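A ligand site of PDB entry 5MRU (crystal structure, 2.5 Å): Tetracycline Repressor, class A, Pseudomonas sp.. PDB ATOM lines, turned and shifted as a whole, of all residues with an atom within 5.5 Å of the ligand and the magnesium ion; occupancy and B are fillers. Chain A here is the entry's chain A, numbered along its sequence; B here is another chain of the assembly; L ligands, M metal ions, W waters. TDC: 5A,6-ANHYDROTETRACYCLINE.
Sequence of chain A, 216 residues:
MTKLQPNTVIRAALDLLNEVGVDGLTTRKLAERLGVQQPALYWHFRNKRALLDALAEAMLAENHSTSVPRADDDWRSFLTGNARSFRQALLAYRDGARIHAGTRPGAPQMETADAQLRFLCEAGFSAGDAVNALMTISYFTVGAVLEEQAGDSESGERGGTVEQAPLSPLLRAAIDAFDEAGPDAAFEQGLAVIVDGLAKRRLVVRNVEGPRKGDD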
ATOM      1  N   LEU A  60      -5.094 -16.301 -11.770  1.00  0.00           N
ATOM      2  CA  LEU A  60      -5.357 -17.539 -12.515  1.00  0.00           C
ATOM      3  C   LEU A  60      -5.926 -18.644 -11.656  1.00  0.00           C
ATOM      4  O   LEU A  60      -6.802 -19.359 -12.066  1.00  0.00           O
ATOM      5  CB  LEU A  60      -4.060 -18.045 -13.184  1.00  0.00           C
ATOM      6  CG  LEU A  60      -3.307 -17.087 -14.145  1.00  0.00           C
ATOM      7  CD1 LEU A  60      -2.173 -17.798 -14.898  1.00  0.00           C
ATOM      8  CD2 LEU A  60      -4.258 -16.389 -15.123  1.00  0.00           C
ATOM      9  N   HIS A  64      -9.025 -18.769 -14.013  1.00  0.00           N
ATOM     10  CA  HIS A  64      -8.607 -19.443 -15.249  1.00  0.00           C
ATOM     11  C   HIS A  64      -9.174 -20.838 -15.256  1.00  0.00           C
ATOM     12  O   HIS A  64      -8.562 -21.779 -14.766  1.00  0.00           O
ATOM     13  CB  HIS A  64      -7.075 -19.478 -15.353  1.00  0.00           C
ATOM     14  CG  HIS A  64      -6.568 -19.949 -16.684  1.00  0.00           C
ATOM     15  ND1 HIS A  64      -7.343 -19.994 -17.816  1.00  0.00           N
ATOM     16  CD2 HIS A  64      -5.334 -20.387 -17.054  1.00  0.00           C
ATOM     17  CE1 HIS A  64      -6.620 -20.445 -18.824  1.00  0.00           C
ATOM     18  NE2 HIS A  64      -5.398 -20.692 -18.386  1.00  0.00           N
ATOM     19  N   SER A  67      -8.177 -23.586 -18.244  1.00  0.00           N
ATOM     20  CA  SER A  67      -6.727 -23.853 -18.188  1.00  0.00           C
ATOM     21  C   SER A  67      -6.345 -25.309 -18.498  1.00  0.00           C
ATOM     22  O   SER A  67      -5.603 -25.581 -19.431  1.00  0.00           O
ATOM     23  CB  SER A  67      -6.211 -23.514 -16.768  1.00  0.00           C
ATOM     24  OG  SER A  67      -5.050 -24.247 -16.384  1.00  0.00           O
ATOM     25  N   ASN A  82      -9.632 -21.921 -23.485  1.00  0.00           N
ATOM     26  CA  ASN A  82      -8.386 -21.565 -22.794  1.00  0.00           C
ATOM     27  C   ASN A  82      -8.034 -20.113 -22.854  1.00  0.00           C
ATOM     28  O   ASN A  82      -7.648 -19.548 -21.865  1.00  0.00           O
ATOM     29  CB  ASN A  82      -7.236 -22.297 -23.416  1.00  0.00           C
ATOM     30  CG  ASN A  82      -5.935 -21.918 -22.825  1.00  0.00           C
ATOM     31  OD1 ASN A  82      -5.092 -21.339 -23.501  1.00  0.00           O
ATOM     32  ND2 ASN A  82      -5.745 -22.265 -21.553  1.00  0.00           N
ATOM     33  N   ALA A  83      -8.177 -19.534 -24.037  1.00  0.00           N
ATOM     34  CA  ALA A  83      -7.894 -18.127 -24.281  1.00  0.00           C
ATOM     35  C   ALA A  83      -8.954 -17.246 -23.665  1.00  0.00           C
ATOM     36  O   ALA A  83      -8.667 -16.212 -23.064  1.00  0.00           O
ATOM     37  CB  ALA A  83      -7.862 -17.872 -25.784  1.00  0.00           C
ATOM     38  N   PHE A  86      -8.316 -17.525 -19.833  1.00  0.00           N
ATOM     39  CA  PHE A  86      -7.151 -16.737 -19.481  1.00  0.00           C
ATOM     40  C   PHE A  86      -7.578 -15.272 -19.403  1.00  0.00           C
ATOM     41  O   PHE A  86      -7.504 -14.657 -18.343  1.00  0.00           O
ATOM     42  CB  PHE A  86      -6.049 -16.945 -20.532  1.00  0.00           C
ATOM     43  CG  PHE A  86      -4.759 -16.192 -20.266  1.00  0.00           C
ATOM     44  CD1 PHE A  86      -4.199 -16.136 -19.010  1.00  0.00           C
ATOM     45  CD2 PHE A  86      -4.074 -15.595 -21.302  1.00  0.00           C
ATOM     46  CE1 PHE A  86      -3.009 -15.479 -18.776  1.00  0.00           C
ATOM     47  CE2 PHE A  86      -2.866 -14.924 -21.085  1.00  0.00           C
ATOM     48  CZ  PHE A  86      -2.344 -14.868 -19.798  1.00  0.00           C
ATOM     49  N   HIS A 100       0.808  -9.558 -15.368  1.00  0.00           N
ATOM     50  CA  HIS A 100       1.147 -10.881 -15.888  1.00  0.00           C
ATOM     51  C   HIS A 100       2.348 -10.868 -16.793  1.00  0.00           C
ATOM     52  O   HIS A 100       3.044 -11.865 -16.942  1.00  0.00           O
ATOM     53  CB  HIS A 100      -0.007 -11.421 -16.706  1.00  0.00           C
ATOM     54  CG  HIS A 100       0.294 -12.740 -17.301  1.00  0.00           C
ATOM     55  ND1 HIS A 100       0.022 -13.912 -16.633  1.00  0.00           N
ATOM     56  CD2 HIS A 100       0.886 -13.087 -18.460  1.00  0.00           C
ATOM     57  CE1 HIS A 100       0.421 -14.938 -17.368  1.00  0.00           C
ATOM     58  NE2 HIS A 100       0.983 -14.463 -18.473  1.00  0.00           N
ATOM     59  N   THR A 103       5.868 -12.665 -16.569  1.00  0.00           N
ATOM     60  CA  THR A 103       5.873 -13.746 -15.608  1.00  0.00           C
ATOM     61  C   THR A 103       6.096 -15.024 -16.386  1.00  0.00           C
ATOM     62  O   THR A 103       5.866 -15.072 -17.587  1.00  0.00           O
ATOM     63  CB  THR A 103       4.580 -13.884 -14.752  1.00  0.00           C
ATOM     64  OG1 THR A 103       3.448 -14.154 -15.584  1.00  0.00           O
ATOM     65  CG2 THR A 103       4.326 -12.631 -13.909  1.00  0.00           C
ATOM     66  N   ARG A 104       6.610 -16.032 -15.710  1.00  0.00           N
ATOM     67  CA  ARG A 104       6.845 -17.335 -16.315  1.00  0.00           C
ATOM     68  C   ARG A 104       6.164 -18.329 -15.414  1.00  0.00           C
ATOM     69  O   ARG A 104       6.346 -18.297 -14.193  1.00  0.00           O
ATOM     70  CB  ARG A 104       8.338 -17.641 -16.472  1.00  0.00           C
ATOM     71  CG  ARG A 104       8.925 -17.275 -17.833  1.00  0.00           C
ATOM     72  CD  ARG A 104       8.388 -15.925 -18.343  1.00  0.00           C
ATOM     73  NE  ARG A 104       8.981 -15.270 -19.515  1.00  0.00           N
ATOM     74  CZ  ARG A 104       9.764 -15.809 -20.447  1.00  0.00           C
ATOM     75  NH1 ARG A 104      10.160 -17.083 -20.433  1.00  0.00           N
ATOM     76  NH2 ARG A 104      10.192 -15.012 -21.427  1.00  0.00           N
ATOM     77  N   PRO A 105       5.358 -19.214 -16.009  1.00  0.00           N
ATOM     78  CA  PRO A 105       4.531 -20.123 -15.221  1.00  0.00           C
ATOM     79  C   PRO A 105       5.375 -20.947 -14.212  1.00  0.00           C
ATOM     80  O   PRO A 105       6.456 -21.431 -14.570  1.00  0.00           O
ATOM     81  CB  PRO A 105       3.865 -20.995 -16.288  1.00  0.00           C
ATOM     82  CG  PRO A 105       4.820 -20.961 -17.454  1.00  0.00           C
ATOM     83  CD  PRO A 105       5.386 -19.579 -17.436  1.00  0.00           C
ATOM     84  N   GLN A 109       2.398 -24.539 -11.955  1.00  0.00           N
ATOM     85  CA  GLN A 109       1.896 -24.118 -13.251  1.00  0.00           C
ATOM     86  C   GLN A 109       2.627 -24.867 -14.390  1.00  0.00           C
ATOM     87  O   GLN A 109       2.114 -24.947 -15.495  1.00  0.00           O
ATOM     88  CB  GLN A 109       2.034 -22.606 -13.409  1.00  0.00           C
ATOM     89  CG  GLN A 109       1.798 -21.815 -12.128  1.00  0.00           C
ATOM     90  N   THR A 112       0.901 -28.630 -14.816  1.00  0.00           N
ATOM     91  CA  THR A 112      -0.316 -28.377 -15.639  1.00  0.00           C
ATOM     92  C   THR A 112      -0.050 -27.769 -17.049  1.00  0.00           C
ATOM     93  O   THR A 112      -0.786 -28.071 -17.993  1.00  0.00           O
ATOM     94  CB  THR A 112      -1.407 -27.530 -14.904  1.00  0.00           C
ATOM     95  OG1 THR A 112      -2.304 -26.969 -15.867  1.00  0.00           O
ATOM     96  CG2 THR A 112      -0.813 -26.394 -14.066  1.00  0.00           C
ATOM     97  N   ALA A 113       0.974 -26.940 -17.200  1.00  0.00           N
ATOM     98  CA  ALA A 113       1.338 -26.424 -18.533  1.00  0.00           C
ATOM     99  C   ALA A 113       1.930 -27.511 -19.458  1.00  0.00           C
ATOM    100  O   ALA A 113       1.857 -27.372 -20.680  1.00  0.00           O
ATOM    101  CB  ALA A 113       2.318 -25.280 -18.408  1.00  0.00           C
ATOM    102  N   GLN A 116      -1.092 -29.299 -21.163  1.00  0.00           N
ATOM    103  CA  GLN A 116      -1.615 -28.535 -22.293  1.00  0.00           C
ATOM    104  C   GLN A 116      -0.977 -29.041 -23.583  1.00  0.00           C
ATOM    105  O   GLN A 116      -1.674 -29.467 -24.516  1.00  0.00           O
ATOM    106  CB  GLN A 116      -1.354 -27.019 -22.134  1.00  0.00           C
ATOM    107  CG  GLN A 116      -1.980 -26.396 -20.902  1.00  0.00           C
ATOM    108  CD  GLN A 116      -2.123 -24.876 -20.987  1.00  0.00           C
ATOM    109  OE1 GLN A 116      -2.396 -24.337 -22.058  1.00  0.00           O
ATOM    110  NE2 GLN A 116      -1.964 -24.185 -19.865  1.00  0.00           N
ATOM    111  N   ALA A 133       1.454 -22.051 -30.697  1.00  0.00           N
ATOM    112  CA  ALA A 133       0.014 -21.867 -30.452  1.00  0.00           C
ATOM    113  C   ALA A 133      -0.292 -21.270 -29.062  1.00  0.00           C
ATOM    114  O   ALA A 133      -1.229 -20.509 -28.892  1.00  0.00           O
ATOM    115  CB  ALA A 133      -0.745 -23.180 -30.647  1.00  0.00           C
ATOM    116  N   LEU A 134       0.498 -21.634 -28.052  1.00  0.00           N
ATOM    117  CA  LEU A 134       0.177 -21.213 -26.705  1.00  0.00           C
ATOM    118  C   LEU A 134       0.732 -19.833 -26.544  1.00  0.00           C
ATOM    119  O   LEU A 134       0.044 -18.928 -26.104  1.00  0.00           O
ATOM    120  CB  LEU A 134       0.738 -22.199 -25.683  1.00  0.00           C
ATOM    121  CG  LEU A 134       0.101 -23.628 -25.770  1.00  0.00           C
ATOM    122  CD1 LEU A 134       0.550 -24.540 -24.640  1.00  0.00           C
ATOM    123  CD2 LEU A 134      -1.423 -23.591 -25.800  1.00  0.00           C
ATOM    124  N   MET A 135       1.973 -19.647 -26.948  1.00  0.00           N
ATOM    125  CA  MET A 135       2.571 -18.337 -26.811  1.00  0.00           C
ATOM    126  C   MET A 135       1.742 -17.294 -27.561  1.00  0.00           C
ATOM    127  O   MET A 135       1.345 -16.280 -27.012  1.00  0.00           O
ATOM    128  CB  MET A 135       4.038 -18.349 -27.291  1.00  0.00           C
ATOM    129  CG  MET A 135       4.999 -17.807 -26.238  1.00  0.00           C
ATOM    130  SD  MET A 135       5.145 -18.855 -24.747  1.00  0.00           S
ATOM    131  CE  MET A 135       6.479 -19.926 -25.321  1.00  0.00           C
ATOM    132  N   ILE A 137      -1.333 -17.105 -28.681  1.00  0.00           N
ATOM    133  CA  ILE A 137      -2.605 -16.850 -28.037  1.00  0.00           C
ATOM    134  C   ILE A 137      -2.350 -16.034 -26.803  1.00  0.00           C
ATOM    135  O   ILE A 137      -3.014 -15.026 -26.562  1.00  0.00           O
ATOM    136  CB  ILE A 137      -3.325 -18.178 -27.686  1.00  0.00           C
ATOM    137  CG1 ILE A 137      -3.884 -18.833 -28.948  1.00  0.00           C
ATOM    138  CG2 ILE A 137      -4.482 -17.966 -26.703  1.00  0.00           C
ATOM    139  CD1 ILE A 137      -4.449 -20.190 -28.717  1.00  0.00           C
ATOM    140  N   SER A 138      -1.360 -16.458 -26.033  1.00  0.00           N
ATOM    141  CA  SER A 138      -0.925 -15.728 -24.855  1.00  0.00           C
ATOM    142  C   SER A 138      -0.533 -14.246 -25.146  1.00  0.00           C
ATOM    143  O   SER A 138      -1.020 -13.292 -24.494  1.00  0.00           O
ATOM    144  CB  SER A 138       0.213 -16.519 -24.243  1.00  0.00           C
ATOM    145  OG  SER A 138       0.744 -15.827 -23.159  1.00  0.00           O
ATOM    146  N   THR A 141      -3.608 -12.212 -26.187  1.00  0.00           N
ATOM    147  CA  THR A 141      -4.577 -11.986 -25.119  1.00  0.00           C
ATOM    148  C   THR A 141      -4.095 -10.850 -24.198  1.00  0.00           C
ATOM    149  O   THR A 141      -4.797  -9.846 -23.978  1.00  0.00           O
ATOM    150  CB  THR A 141      -4.749 -13.274 -24.319  1.00  0.00           C
ATOM    151  OG1 THR A 141      -4.997 -14.342 -25.229  1.00  0.00           O
ATOM    152  CG2 THR A 141      -5.898 -13.197 -23.343  1.00  0.00           C
ATOM    153  N   GLU B 147       5.641  -8.448 -23.130  1.00  0.00           N
ATOM    154  CA  GLU B 147       6.190  -9.593 -22.423  1.00  0.00           C
ATOM    155  C   GLU B 147       7.682  -9.586 -22.583  1.00  0.00           C
ATOM    156  O   GLU B 147       8.419  -9.795 -21.621  1.00  0.00           O
ATOM    157  CB  GLU B 147       5.585 -10.899 -22.876  1.00  0.00           C
ATOM    158  CG  GLU B 147       4.085 -11.013 -22.573  1.00  0.00           C
ATOM    159  CD  GLU B 147       3.821 -11.969 -21.439  1.00  0.00           C
ATOM    160  OE1 GLU B 147       4.749 -12.165 -20.631  1.00  0.00           O
ATOM    161  OE2 GLU B 147       2.698 -12.534 -21.368  1.00  0.00           O
HETATM  162  O12 TDC L   1       1.108 -16.953 -19.625  1.00  0.00           O
HETATM  163  C12 TDC L   1       1.058 -18.121 -20.104  1.00  0.00           C
HETATM  164  C1B TDC L   1       2.294 -18.790 -20.580  1.00  0.00           C
HETATM  165  C11 TDC L   1       3.506 -18.139 -20.423  1.00  0.00           C
HETATM  166  O11 TDC L   1       3.573 -16.882 -19.852  1.00  0.00           O
HETATM  167  C1A TDC L   1       4.682 -18.743 -20.838  1.00  0.00           C
HETATM  168  C10 TDC L   1       5.893 -18.078 -20.682  1.00  0.00           C
HETATM  169  O10 TDC L   1       5.998 -16.812 -20.121  1.00  0.00           O
HETATM  170  C9  TDC L   1       7.133 -18.729 -21.127  1.00  0.00           C
HETATM  171  C8  TDC L   1       7.054 -19.993 -21.681  1.00  0.00           C
HETATM  172  C7  TDC L   1       5.824 -20.607 -21.815  1.00  0.00           C
HETATM  173  C61 TDC L   1       4.632 -20.013 -21.414  1.00  0.00           C
HETATM  174  C6  TDC L   1       3.387 -20.666 -21.560  1.00  0.00           C
HETATM  175  C62 TDC L   1       3.252 -22.031 -22.164  1.00  0.00           C
HETATM  176  C51 TDC L   1       2.209 -20.061 -21.135  1.00  0.00           C
HETATM  177  C5  TDC L   1       0.885 -20.759 -21.322  1.00  0.00           C
HETATM  178  C1C TDC L   1      -0.222 -18.902 -20.157  1.00  0.00           C
HETATM  179  C1  TDC L   1      -0.284 -19.898 -18.992  1.00  0.00           C
HETATM  180  O1  TDC L   1       0.603 -19.886 -18.139  1.00  0.00           O
HETATM  181  O1C TDC L   1      -1.351 -18.069 -20.194  1.00  0.00           O
HETATM  182  C41 TDC L   1      -0.276 -19.766 -21.381  1.00  0.00           C
HETATM  183  C4  TDC L   1      -1.631 -20.535 -21.540  1.00  0.00           C
HETATM  184  N4  TDC L   1      -2.709 -19.967 -22.441  1.00  0.00           N
HETATM  185  C43 TDC L   1      -2.837 -18.486 -22.434  1.00  0.00           C
HETATM  186  C42 TDC L   1      -2.343 -20.404 -23.836  1.00  0.00           C
HETATM  187  C3  TDC L   1      -2.184 -21.005 -20.182  1.00  0.00           C
HETATM  188  O3  TDC L   1      -3.189 -21.687 -20.225  1.00  0.00           O
HETATM  189  C2  TDC L   1      -1.457 -20.755 -18.955  1.00  0.00           C
HETATM  190  C21 TDC L   1      -1.917 -21.326 -17.678  1.00  0.00           C
HETATM  191  O21 TDC L   1      -2.879 -22.106 -17.658  1.00  0.00           O
HETATM  192  N21 TDC L   1      -1.236 -21.130 -16.533  1.00  0.00           N
HETATM  193 MG    MG M   1       2.854 -15.757 -18.445  1.00  0.00          MG
HETATM  194  O   HOH W   1       4.113 -14.373 -19.280  1.00  0.00           O
HETATM  195  O   HOH W   2       2.064 -17.569 -17.002  1.00  0.00           O
HETATM  196  O   HOH W   3       2.121 -15.121 -21.026  1.00  0.00           O
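The backbone carbonyl oxygen of Thr 103 sits at hydrogen-bond distance from an oxygen (O10) of the ligand, at 3.1 Å. A ring nitrogen (NE2) of His 64 lies within hydrogen-bond range of an oxygen (O21) of the ligand. The guanidinium group (NE) of Arg 104 sits close to an oxygen (O10) of the ligand, 3.4 Å away. OG of Ser 67 is in hydrogen-bond range of O21 of the ligand. The side-chain amide nitrogen of Gln 116 lies within hydrogen-bond range of an oxygen (O3) of the ligand, at 2.8 Å. The side-chain amide nitrogen of Asn 82 sits at hydrogen-bond distance from an oxygen (O3) of the ligand, 2.9 Å away.
A ring nitrogen (ND1) of His 64 lies within hydrogen-bond range of the backbone NH of Phe 86, 3.3 Å away. The backbone carbonyl oxygen of His 100 lies within hydrogen-bond range of the side-chain hydroxyl of Thr 103 (2.7 Å).
Merely in contact with the ligand: Phe 86, Met 135, Pro 105, Leu 134, Ser 138 and Leu 60. Hydrophobic or aromatic side chains that line the ligand: Leu 60, His 64, Phe 86, His 100, Pro 105, Leu 134 and Met 135. Of the 21 residues printed, 13 come within 4 Å of the ligand. Along chain A the residues within 4 Å of the ligand span positions 60 to 138.
Merely in contact with the magnesium ion: Thr 103 (3.2 Å). Of the 21 residues printed, 2 come within 4 Å of the magnesium ion.
The magnesium ion is bound by O11 of the ligand (1.9 Å), water W1 (2.0 Å), NE2 of His 100 (2.3 Å), O12 of the ligand (2.4 Å) and water W2 (2.4 Å). Slightly farther from the magnesium ion lies water W3 (2.8 Å).
Water W1 lies within hydrogen-bond range of the backbone carbonyl oxygen (O) of Thr 103 (2.5 Å), the side-chain carboxylate (OE1) of Glu 147 of chain B (2.7 Å) and an oxygen (O10) of the ligand (3.2 Å). Water W3 lies within hydrogen-bond range of the side-chain hydroxyl (OG) of Ser 138 (2.6 Å) and the side-chain carboxylate (OE2) of Glu 147 of chain B (2.7 Å).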
